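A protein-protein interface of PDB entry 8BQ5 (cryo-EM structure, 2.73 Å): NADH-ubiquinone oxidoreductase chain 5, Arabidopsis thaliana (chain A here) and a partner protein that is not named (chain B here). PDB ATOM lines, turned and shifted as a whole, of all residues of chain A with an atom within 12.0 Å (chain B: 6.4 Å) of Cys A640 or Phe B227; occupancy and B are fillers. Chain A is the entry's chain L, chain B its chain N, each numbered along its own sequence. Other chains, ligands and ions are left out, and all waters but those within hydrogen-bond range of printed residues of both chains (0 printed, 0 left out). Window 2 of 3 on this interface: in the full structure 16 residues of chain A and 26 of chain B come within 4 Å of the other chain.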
ATOM      1  N   GLY A 631     -11.598  -8.316  -5.333  1.00  0.00           N
ATOM      2  CA  GLY A 631     -11.371  -9.587  -4.668  1.00  0.00           C
ATOM      3  C   GLY A 631     -12.036 -10.742  -5.389  1.00  0.00           C
ATOM      4  O   GLY A 631     -11.443 -11.810  -5.552  1.00  0.00           O
ATOM      5  N   LEU A 632     -13.277 -10.539  -5.839  1.00  0.00           N
ATOM      6  CA  LEU A 632     -13.949 -11.559  -6.640  1.00  0.00           C
ATOM      7  C   LEU A 632     -13.189 -11.836  -7.935  1.00  0.00           C
ATOM      8  O   LEU A 632     -13.019 -12.998  -8.332  1.00  0.00           O
ATOM      9  CB  LEU A 632     -15.382 -11.120  -6.937  1.00  0.00           C
ATOM     10  CG  LEU A 632     -16.259 -12.026  -7.804  1.00  0.00           C
ATOM     11  CD1 LEU A 632     -16.566 -13.339  -7.105  1.00  0.00           C
ATOM     12  CD2 LEU A 632     -17.540 -11.303  -8.184  1.00  0.00           C
ATOM     13  N   THR A 633     -12.723 -10.779  -8.606  1.00  0.00           N
ATOM     14  CA  THR A 633     -11.967 -10.955  -9.842  1.00  0.00           C
ATOM     15  C   THR A 633     -10.664 -11.703  -9.595  1.00  0.00           C
ATOM     16  O   THR A 633     -10.284 -12.578 -10.380  1.00  0.00           O
ATOM     17  CB  THR A 633     -11.683  -9.600 -10.487  1.00  0.00           C
ATOM     18  OG1 THR A 633     -12.906  -8.867 -10.620  1.00  0.00           O
ATOM     19  CG2 THR A 633     -11.063  -9.786 -11.862  1.00  0.00           C
ATOM     20  N   LEU A 634      -9.957 -11.362  -8.514  1.00  0.00           N
ATOM     21  CA  LEU A 634      -8.721 -12.061  -8.183  1.00  0.00           C
ATOM     22  C   LEU A 634      -8.990 -13.528  -7.884  1.00  0.00           C
ATOM     23  O   LEU A 634      -8.232 -14.405  -8.318  1.00  0.00           O
ATOM     24  CB  LEU A 634      -8.033 -11.386  -6.997  1.00  0.00           C
ATOM     25  CG  LEU A 634      -6.759 -12.060  -6.481  1.00  0.00           C
ATOM     26  CD1 LEU A 634      -5.588 -11.754  -7.399  1.00  0.00           C
ATOM     27  CD2 LEU A 634      -6.450 -11.626  -5.057  1.00  0.00           C
ATOM     28  N   PHE A 635     -10.067 -13.815  -7.149  1.00  0.00           N
ATOM     29  CA  PHE A 635     -10.430 -15.202  -6.877  1.00  0.00           C
ATOM     30  C   PHE A 635     -10.639 -15.970  -8.171  1.00  0.00           C
ATOM     31  O   PHE A 635     -10.047 -17.038  -8.376  1.00  0.00           O
ATOM     32  CB  PHE A 635     -11.696 -15.255  -6.023  1.00  0.00           C
ATOM     33  CG  PHE A 635     -11.435 -15.218  -4.552  1.00  0.00           C
ATOM     34  CD1 PHE A 635     -10.213 -14.798  -4.062  1.00  0.00           C
ATOM     35  CD2 PHE A 635     -12.412 -15.613  -3.655  1.00  0.00           C
ATOM     36  CE1 PHE A 635      -9.971 -14.764  -2.706  1.00  0.00           C
ATOM     37  CE2 PHE A 635     -12.175 -15.583  -2.298  1.00  0.00           C
ATOM     38  CZ  PHE A 635     -10.954 -15.157  -1.824  1.00  0.00           C
ATOM     39  N   VAL A 636     -11.469 -15.429  -9.065  1.00  0.00           N
ATOM     40  CA  VAL A 636     -11.752 -16.110 -10.326  1.00  0.00           C
ATOM     41  C   VAL A 636     -10.465 -16.322 -11.115  1.00  0.00           C
ATOM     42  O   VAL A 636     -10.165 -17.437 -11.562  1.00  0.00           O
ATOM     43  CB  VAL A 636     -12.786 -15.316 -11.146  1.00  0.00           C
ATOM     44  CG1 VAL A 636     -12.721 -15.720 -12.609  1.00  0.00           C
ATOM     45  CG2 VAL A 636     -14.186 -15.522 -10.589  1.00  0.00           C
ATOM     46  N   THR A 637      -9.670 -15.259 -11.266  1.00  0.00           N
ATOM     47  CA  THR A 637      -8.487 -15.322 -12.119  1.00  0.00           C
ATOM     48  C   THR A 637      -7.461 -16.309 -11.578  1.00  0.00           C
ATOM     49  O   THR A 637      -6.861 -17.073 -12.341  1.00  0.00           O
ATOM     50  CB  THR A 637      -7.859 -13.935 -12.261  1.00  0.00           C
ATOM     51  OG1 THR A 637      -7.986 -13.218 -11.029  1.00  0.00           O
ATOM     52  CG2 THR A 637      -8.534 -13.152 -13.372  1.00  0.00           C
ATOM     53  N   PHE A 638      -7.224 -16.300 -10.267  1.00  0.00           N
ATOM     54  CA  PHE A 638      -6.184 -17.169  -9.732  1.00  0.00           C
ATOM     55  C   PHE A 638      -6.653 -18.615  -9.667  1.00  0.00           C
ATOM     56  O   PHE A 638      -5.899 -19.531 -10.011  1.00  0.00           O
ATOM     57  CB  PHE A 638      -5.735 -16.675  -8.357  1.00  0.00           C
ATOM     58  CG  PHE A 638      -4.746 -17.584  -7.674  1.00  0.00           C
ATOM     59  CD1 PHE A 638      -5.168 -18.624  -6.859  1.00  0.00           C
ATOM     60  CD2 PHE A 638      -3.386 -17.397  -7.859  1.00  0.00           C
ATOM     61  CE1 PHE A 638      -4.250 -19.452  -6.238  1.00  0.00           C
ATOM     62  CE2 PHE A 638      -2.467 -18.222  -7.242  1.00  0.00           C
ATOM     63  CZ  PHE A 638      -2.898 -19.249  -6.431  1.00  0.00           C
ATOM     64  N   PHE A 639      -7.893 -18.849  -9.241  1.00  0.00           N
ATOM     65  CA  PHE A 639      -8.338 -20.208  -8.988  1.00  0.00           C
ATOM     66  C   PHE A 639      -8.940 -20.882 -10.214  1.00  0.00           C
ATOM     67  O   PHE A 639      -9.273 -22.069 -10.144  1.00  0.00           O
ATOM     68  CB  PHE A 639      -9.334 -20.200  -7.826  1.00  0.00           C
ATOM     69  CG  PHE A 639      -8.676 -20.186  -6.470  1.00  0.00           C
ATOM     70  CD1 PHE A 639      -9.026 -19.240  -5.523  1.00  0.00           C
ATOM     71  CD2 PHE A 639      -7.730 -21.143  -6.133  1.00  0.00           C
ATOM     72  CE1 PHE A 639      -8.417 -19.223  -4.282  1.00  0.00           C
ATOM     73  CE2 PHE A 639      -7.131 -21.139  -4.885  1.00  0.00           C
ATOM     74  CZ  PHE A 639      -7.478 -20.180  -3.957  1.00  0.00           C
ATOM     75  N   CYS A 640      -9.096 -20.164 -11.325  1.00  0.00           N
ATOM     76  CA  CYS A 640      -9.499 -20.834 -12.557  1.00  0.00           C
ATOM     77  C   CYS A 640      -8.632 -20.460 -13.750  1.00  0.00           C
ATOM     78  O   CYS A 640      -8.374 -21.311 -14.606  1.00  0.00           O
ATOM     79  CB  CYS A 640     -10.967 -20.520 -12.859  1.00  0.00           C
ATOM     80  SG  CYS A 640     -12.124 -21.181 -11.637  1.00  0.00           S
ATOM     81  N   MET A 641      -8.187 -19.208 -13.834  1.00  0.00           N
ATOM     82  CA  MET A 641      -7.412 -18.715 -14.973  1.00  0.00           C
ATOM     83  C   MET A 641      -5.912 -18.841 -14.702  1.00  0.00           C
ATOM     84  O   MET A 641      -5.128 -17.918 -14.911  1.00  0.00           O
ATOM     85  CB  MET A 641      -7.794 -17.269 -15.262  1.00  0.00           C
ATOM     86  CG  MET A 641      -7.871 -16.885 -16.715  1.00  0.00           C
ATOM     87  SD  MET A 641      -8.653 -15.268 -16.887  1.00  0.00           S
ATOM     88  CE  MET A 641      -7.218 -14.196 -16.883  1.00  0.00           C
ATOM     89  N   TRP A 642      -5.512 -20.028 -14.256  1.00  0.00           N
ATOM     90  CA  TRP A 642      -4.112 -20.305 -13.959  1.00  0.00           C
ATOM     91  C   TRP A 642      -3.717 -21.648 -14.556  1.00  0.00           C
ATOM     92  O   TRP A 642      -2.774 -22.304 -14.099  1.00  0.00           O
ATOM     93  CB  TRP A 642      -3.849 -20.238 -12.453  1.00  0.00           C
ATOM     94  CG  TRP A 642      -2.502 -19.663 -12.103  1.00  0.00           C
ATOM     95  CD1 TRP A 642      -1.358 -20.360 -11.854  1.00  0.00           C
ATOM     96  CD2 TRP A 642      -2.146 -18.272 -12.033  1.00  0.00           C
ATOM     97  NE1 TRP A 642      -0.321 -19.497 -11.595  1.00  0.00           N
ATOM     98  CE2 TRP A 642      -0.778 -18.209 -11.704  1.00  0.00           C
ATOM     99  CE3 TRP A 642      -2.854 -17.078 -12.205  1.00  0.00           C
ATOM    100  CZ2 TRP A 642      -0.102 -17.001 -11.543  1.00  0.00           C
ATOM    101  CZ3 TRP A 642      -2.180 -15.878 -12.044  1.00  0.00           C
ATOM    102  CH2 TRP A 642      -0.819 -15.849 -11.716  1.00  0.00           C
ATOM    103  N   ASP A 643      -4.435 -22.058 -15.603  1.00  0.00           N
ATOM    104  CA  ASP A 643      -4.163 -23.293 -16.333  1.00  0.00           C
ATOM    105  C   ASP A 643      -3.092 -23.096 -17.400  1.00  0.00           C
ATOM    106  O   ASP A 643      -2.057 -23.770 -17.382  1.00  0.00           O
ATOM    107  CB  ASP A 643      -5.457 -23.814 -16.975  1.00  0.00           C
ATOM    108  CG  ASP A 643      -6.431 -24.370 -15.958  1.00  0.00           C
ATOM    109  OD1 ASP A 643      -5.975 -24.843 -14.896  1.00  0.00           O
ATOM    110  OD2 ASP A 643      -7.652 -24.335 -16.221  1.00  0.00           O
ATOM    111  N   SER A 644      -3.327 -22.187 -18.343  1.00  0.00           N
ATOM    112  CA  SER A 644      -2.372 -21.915 -19.409  1.00  0.00           C
ATOM    113  C   SER A 644      -1.513 -20.687 -19.142  1.00  0.00           C
ATOM    114  O   SER A 644      -0.716 -20.310 -20.007  1.00  0.00           O
ATOM    115  CB  SER A 644      -3.100 -21.754 -20.747  1.00  0.00           C
ATOM    116  OG  SER A 644      -3.749 -22.956 -21.126  1.00  0.00           O
ATOM    117  N   LEU A 645      -1.656 -20.049 -17.979  1.00  0.00           N
ATOM    118  CA  LEU A 645      -0.790 -18.920 -17.661  1.00  0.00           C
ATOM    119  C   LEU A 645       0.600 -19.380 -17.243  1.00  0.00           C
ATOM    120  O   LEU A 645       1.567 -18.623 -17.380  1.00  0.00           O
ATOM    121  CB  LEU A 645      -1.412 -18.060 -16.563  1.00  0.00           C
ATOM    122  CG  LEU A 645      -2.513 -17.093 -17.001  1.00  0.00           C
ATOM    123  CD1 LEU A 645      -2.703 -15.993 -15.968  1.00  0.00           C
ATOM    124  CD2 LEU A 645      -2.204 -16.505 -18.369  1.00  0.00           C
ATOM    125  N   SER A 646       0.722 -20.612 -16.743  1.00  0.00           N
ATOM    126  CA  SER A 646       2.006 -21.097 -16.251  1.00  0.00           C
ATOM    127  C   SER A 646       3.057 -21.192 -17.349  1.00  0.00           C
ATOM    128  O   SER A 646       4.253 -21.231 -17.044  1.00  0.00           O
ATOM    129  CB  SER A 646       1.824 -22.456 -15.576  1.00  0.00           C
ATOM    130  OG  SER A 646       0.734 -22.426 -14.670  1.00  0.00           O
ATOM    131  N   SER A 647       2.643 -21.228 -18.619  1.00  0.00           N
ATOM    132  CA  SER A 647       3.613 -21.254 -19.708  1.00  0.00           C
ATOM    133  C   SER A 647       4.356 -19.928 -19.824  1.00  0.00           C
ATOM    134  O   SER A 647       5.483 -19.884 -20.329  1.00  0.00           O
ATOM    135  CB  SER A 647       2.917 -21.598 -21.025  1.00  0.00           C
ATOM    136  OG  SER A 647       2.367 -22.901 -20.983  1.00  0.00           O
ATOM    137  N   VAL A 649       4.350 -17.555 -16.988  1.00  0.00           N
ATOM    138  CA  VAL A 649       4.582 -16.997 -15.667  1.00  0.00           C
ATOM    139  C   VAL A 649       5.393 -17.978 -14.828  1.00  0.00           C
ATOM    140  O   VAL A 649       5.598 -19.135 -15.195  1.00  0.00           O
ATOM    141  CB  VAL A 649       3.265 -16.637 -14.956  1.00  0.00           C
ATOM    142  CG1 VAL A 649       2.345 -15.872 -15.892  1.00  0.00           C
ATOM    143  CG2 VAL A 649       2.591 -17.897 -14.430  1.00  0.00           C
ATOM    144  N   ILE B 218     -11.844 -31.991  -8.548  1.00  0.00           N
ATOM    145  CA  ILE B 218     -11.334 -31.607  -9.863  1.00  0.00           C
ATOM    146  C   ILE B 218     -10.682 -32.812 -10.529  1.00  0.00           C
ATOM    147  O   ILE B 218      -9.489 -33.072 -10.333  1.00  0.00           O
ATOM    148  CB  ILE B 218     -10.336 -30.439  -9.767  1.00  0.00           C
ATOM    149  CG1 ILE B 218     -10.832 -29.375  -8.788  1.00  0.00           C
ATOM    150  CG2 ILE B 218     -10.086 -29.841 -11.143  1.00  0.00           C
ATOM    151  CD1 ILE B 218      -9.857 -28.234  -8.591  1.00  0.00           C
ATOM    152  N   ARG B 222     -13.849 -30.970 -15.160  1.00  0.00           N
ATOM    153  CA  ARG B 222     -14.405 -30.273 -14.010  1.00  0.00           C
ATOM    154  C   ARG B 222     -15.545 -29.356 -14.429  1.00  0.00           C
ATOM    155  O   ARG B 222     -15.403 -28.544 -15.349  1.00  0.00           O
ATOM    156  CB  ARG B 222     -13.320 -29.457 -13.305  1.00  0.00           C
ATOM    157  CG  ARG B 222     -13.876 -28.412 -12.356  1.00  0.00           C
ATOM    158  CD  ARG B 222     -12.823 -27.437 -11.870  1.00  0.00           C
ATOM    159  NE  ARG B 222     -12.547 -26.406 -12.864  1.00  0.00           N
ATOM    160  CZ  ARG B 222     -11.557 -25.528 -12.779  1.00  0.00           C
ATOM    161  NH1 ARG B 222     -10.755 -25.489 -11.728  1.00  0.00           N
ATOM    162  NH2 ARG B 222     -11.373 -24.661 -13.770  1.00  0.00           N
ATOM    163  N   SER B 223     -16.676 -29.486 -13.741  1.00  0.00           N
ATOM    164  CA  SER B 223     -17.823 -28.612 -13.969  1.00  0.00           C
ATOM    165  C   SER B 223     -17.443 -27.201 -13.548  1.00  0.00           C
ATOM    166  O   SER B 223     -17.308 -26.905 -12.360  1.00  0.00           O
ATOM    167  CB  SER B 223     -19.039 -29.108 -13.194  1.00  0.00           C
ATOM    168  OG  SER B 223     -20.173 -28.297 -13.452  1.00  0.00           O
ATOM    169  N   SER B 224     -17.250 -26.323 -14.532  1.00  0.00           N
ATOM    170  CA  SER B 224     -16.898 -24.943 -14.225  1.00  0.00           C
ATOM    171  C   SER B 224     -18.043 -24.221 -13.524  1.00  0.00           C
ATOM    172  O   SER B 224     -17.808 -23.295 -12.736  1.00  0.00           O
ATOM    173  CB  SER B 224     -16.487 -24.223 -15.507  1.00  0.00           C
ATOM    174  OG  SER B 224     -17.607 -23.661 -16.161  1.00  0.00           O
ATOM    175  N   GLY B 225     -19.282 -24.649 -13.781  1.00  0.00           N
ATOM    176  CA  GLY B 225     -20.418 -24.065 -13.087  1.00  0.00           C
ATOM    177  C   GLY B 225     -20.389 -24.329 -11.594  1.00  0.00           C
ATOM    178  O   GLY B 225     -20.646 -23.433 -10.789  1.00  0.00           O
ATOM    179  N   ILE B 226     -20.072 -25.565 -11.204  1.00  0.00           N
ATOM    180  CA  ILE B 226     -19.975 -25.886  -9.783  1.00  0.00           C
ATOM    181  C   ILE B 226     -18.827 -25.117  -9.140  1.00  0.00           C
ATOM    182  O   ILE B 226     -18.960 -24.591  -8.027  1.00  0.00           O
ATOM    183  CB  ILE B 226     -19.825 -27.404  -9.582  1.00  0.00           C
ATOM    184  CG1 ILE B 226     -21.040 -28.138 -10.138  1.00  0.00           C
ATOM    185  CG2 ILE B 226     -19.686 -27.728  -8.112  1.00  0.00           C
ATOM    186  CD1 ILE B 226     -20.911 -29.642 -10.098  1.00  0.00           C
ATOM    187  N   PHE B 227     -17.684 -25.042  -9.829  1.00  0.00           N
ATOM    188  CA  PHE B 227     -16.554 -24.266  -9.324  1.00  0.00           C
ATOM    189  C   PHE B 227     -16.938 -22.820  -9.047  1.00  0.00           C
ATOM    190  O   PHE B 227     -16.710 -22.313  -7.942  1.00  0.00           O
ATOM    191  CB  PHE B 227     -15.398 -24.307 -10.322  1.00  0.00           C
ATOM    192  CG  PHE B 227     -14.043 -24.252  -9.682  1.00  0.00           C
ATOM    193  CD1 PHE B 227     -13.469 -25.376  -9.133  1.00  0.00           C
ATOM    194  CD2 PHE B 227     -13.348 -23.058  -9.623  1.00  0.00           C
ATOM    195  CE1 PHE B 227     -12.224 -25.323  -8.543  1.00  0.00           C
ATOM    196  CE2 PHE B 227     -12.105 -22.996  -9.037  1.00  0.00           C
ATOM    197  CZ  PHE B 227     -11.540 -24.133  -8.497  1.00  0.00           C
ATOM    198  N   MET B 228     -17.517 -22.137 -10.034  1.00  0.00           N
ATOM    199  CA  MET B 228     -17.863 -20.735  -9.826  1.00  0.00           C
ATOM    200  C   MET B 228     -19.013 -20.548  -8.846  1.00  0.00           C
ATOM    201  O   MET B 228     -19.047 -19.535  -8.139  1.00  0.00           O
ATOM    202  CB  MET B 228     -18.169 -20.060 -11.161  1.00  0.00           C
ATOM    203  CG  MET B 228     -17.054 -20.236 -12.163  1.00  0.00           C
ATOM    204  SD  MET B 228     -15.857 -18.913 -11.910  1.00  0.00           S
ATOM    205  CE  MET B 228     -14.394 -19.620 -12.641  1.00  0.00           C
ATOM    206  N   GLY B 229     -19.950 -21.493  -8.771  1.00  0.00           N
ATOM    207  CA  GLY B 229     -20.960 -21.414  -7.731  1.00  0.00           C
ATOM    208  C   GLY B 229     -20.346 -21.453  -6.347  1.00  0.00           C
ATOM    209  O   GLY B 229     -20.670 -20.632  -5.481  1.00  0.00           O
ATOM    210  N   ILE B 230     -19.422 -22.395  -6.133  1.00  0.00           N
ATOM    211  CA  ILE B 230     -18.703 -22.477  -4.863  1.00  0.00           C
ATOM    212  C   ILE B 230     -17.954 -21.178  -4.599  1.00  0.00           C
ATOM    213  O   ILE B 230     -17.966 -20.649  -3.483  1.00  0.00           O
ATOM    214  CB  ILE B 230     -17.748 -23.686  -4.862  1.00  0.00           C
ATOM    215  CG1 ILE B 230     -18.518 -25.005  -4.807  1.00  0.00           C
ATOM    216  CG2 ILE B 230     -16.790 -23.608  -3.687  1.00  0.00           C
ATOM    217  CD1 ILE B 230     -19.789 -24.941  -4.016  1.00  0.00           C
ATOM    218  N   LEU B 231     -17.295 -20.647  -5.630  1.00  0.00           N
ATOM    219  CA  LEU B 231     -16.507 -19.425  -5.484  1.00  0.00           C
ATOM    220  C   LEU B 231     -17.370 -18.251  -5.030  1.00  0.00           C
ATOM    221  O   LEU B 231     -17.022 -17.531  -4.085  1.00  0.00           O
ATOM    222  CB  LEU B 231     -15.828 -19.102  -6.815  1.00  0.00           C
ATOM    223  CG  LEU B 231     -14.383 -18.611  -6.847  1.00  0.00           C
ATOM    224  CD1 LEU B 231     -13.595 -19.238  -5.730  1.00  0.00           C
ATOM    225  CD2 LEU B 231     -13.744 -18.931  -8.191  1.00  0.00           C
ATOM    226  N   PHE B 232     -18.504 -18.039  -5.702  1.00  0.00           N
ATOM    227  CA  PHE B 232     -19.352 -16.891  -5.392  1.00  0.00           C
ATOM    228  C   PHE B 232     -20.007 -17.043  -4.021  1.00  0.00           C
ATOM    229  O   PHE B 232     -20.108 -16.067  -3.255  1.00  0.00           O
ATOM    230  CB  PHE B 232     -20.397 -16.716  -6.495  1.00  0.00           C
ATOM    231  CG  PHE B 232     -19.887 -15.972  -7.704  1.00  0.00           C
ATOM    232  CD1 PHE B 232     -18.779 -16.432  -8.401  1.00  0.00           C
ATOM    233  CD2 PHE B 232     -20.527 -14.832  -8.157  1.00  0.00           C
ATOM    234  CE1 PHE B 232     -18.310 -15.758  -9.512  1.00  0.00           C
ATOM    235  CE2 PHE B 232     -20.063 -14.154  -9.271  1.00  0.00           C
ATOM    236  CZ  PHE B 232     -18.952 -14.619  -9.949  1.00  0.00           C
ATOM    237  N   GLY B 287     -12.464 -29.707  -4.201  1.00  0.00           N
ATOM    238  CA  GLY B 287     -11.000 -29.729  -4.032  1.00  0.00           C
ATOM    239  C   GLY B 287     -10.523 -28.844  -2.895  1.00  0.00           C
ATOM    240  O   GLY B 287     -11.358 -28.156  -2.264  1.00  0.00           O
ATOM    241  N   THR B 289      -9.429 -26.240  -3.207  1.00  0.00           N
ATOM    242  CA  THR B 289      -9.516 -24.853  -3.666  1.00  0.00           C
ATOM    243  C   THR B 289     -10.145 -23.951  -2.608  1.00  0.00           C
ATOM    244  O   THR B 289      -9.638 -22.863  -2.314  1.00  0.00           O
ATOM    245  CB  THR B 289     -10.323 -24.786  -4.965  1.00  0.00           C
ATOM    246  OG1 THR B 289      -9.484 -25.135  -6.073  1.00  0.00           O
ATOM    247  CG2 THR B 289     -10.885 -23.384  -5.176  1.00  0.00           C
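Printed residues of chain B within 4 Å of Leu A632: Phe B232 (3.8 Å). Printed residues of chain B within 4 Å of Phe A639: Phe B227 and Thr B289. Printed residues of chain B within 4 Å of Cys A640: Phe B227 and Met B228. No residue of chain A comes within 4 Å of Ser B224. No residue of chain A comes within 4 Å of Gly B225. No residue of chain A comes within 4 Å of Ile B226. Of the printed residues of chain A, Met B228 touches Cys A640 (2.9 Å). No residue of chain A comes within 4 Å of Gly B229. No residue of chain A comes within 4 Å of Ile B230. Printed residues of chain A within 4 Å of Phe B232: Leu A632. No residue of chain A comes within 4 Å of Gly B287. Of the printed residues of chain A, Thr B289 touches Phe A639 (3.8 Å). The nearest printed residue of chain B that does not touch Phe A639 is Arg B222 (4.05 Å).
Of the 14 printed residues of chain B, 4 touch a printed residue of chain A. Of the 18 printed residues of chain A, 3 touch a printed residue of chain B. Hydrophobic or aromatic side chains of chain A that line the printed part of chain B: Leu A632 and Phe A639. Among the printed residues, 5 pairs touch across the chains. Among the printed residues, no Asp or Glu carboxylate lies within 4 Å of a Lys or Arg side-chain nitrogen of the other chain.
CD1 of Leu A632 touches CE1 of Phe B232, at 3.8 Å. CE2 of Phe B227 touches O of Phe A639, 3.2 Å away. Phe A639 touches Thr B289 (CZ to O, 3.8 Å). CD2 of Phe B227 touches SG of Cys A640, at 3.0 Å. Cys A640 touches Met B228 (SG to CE, 2.9 Å).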
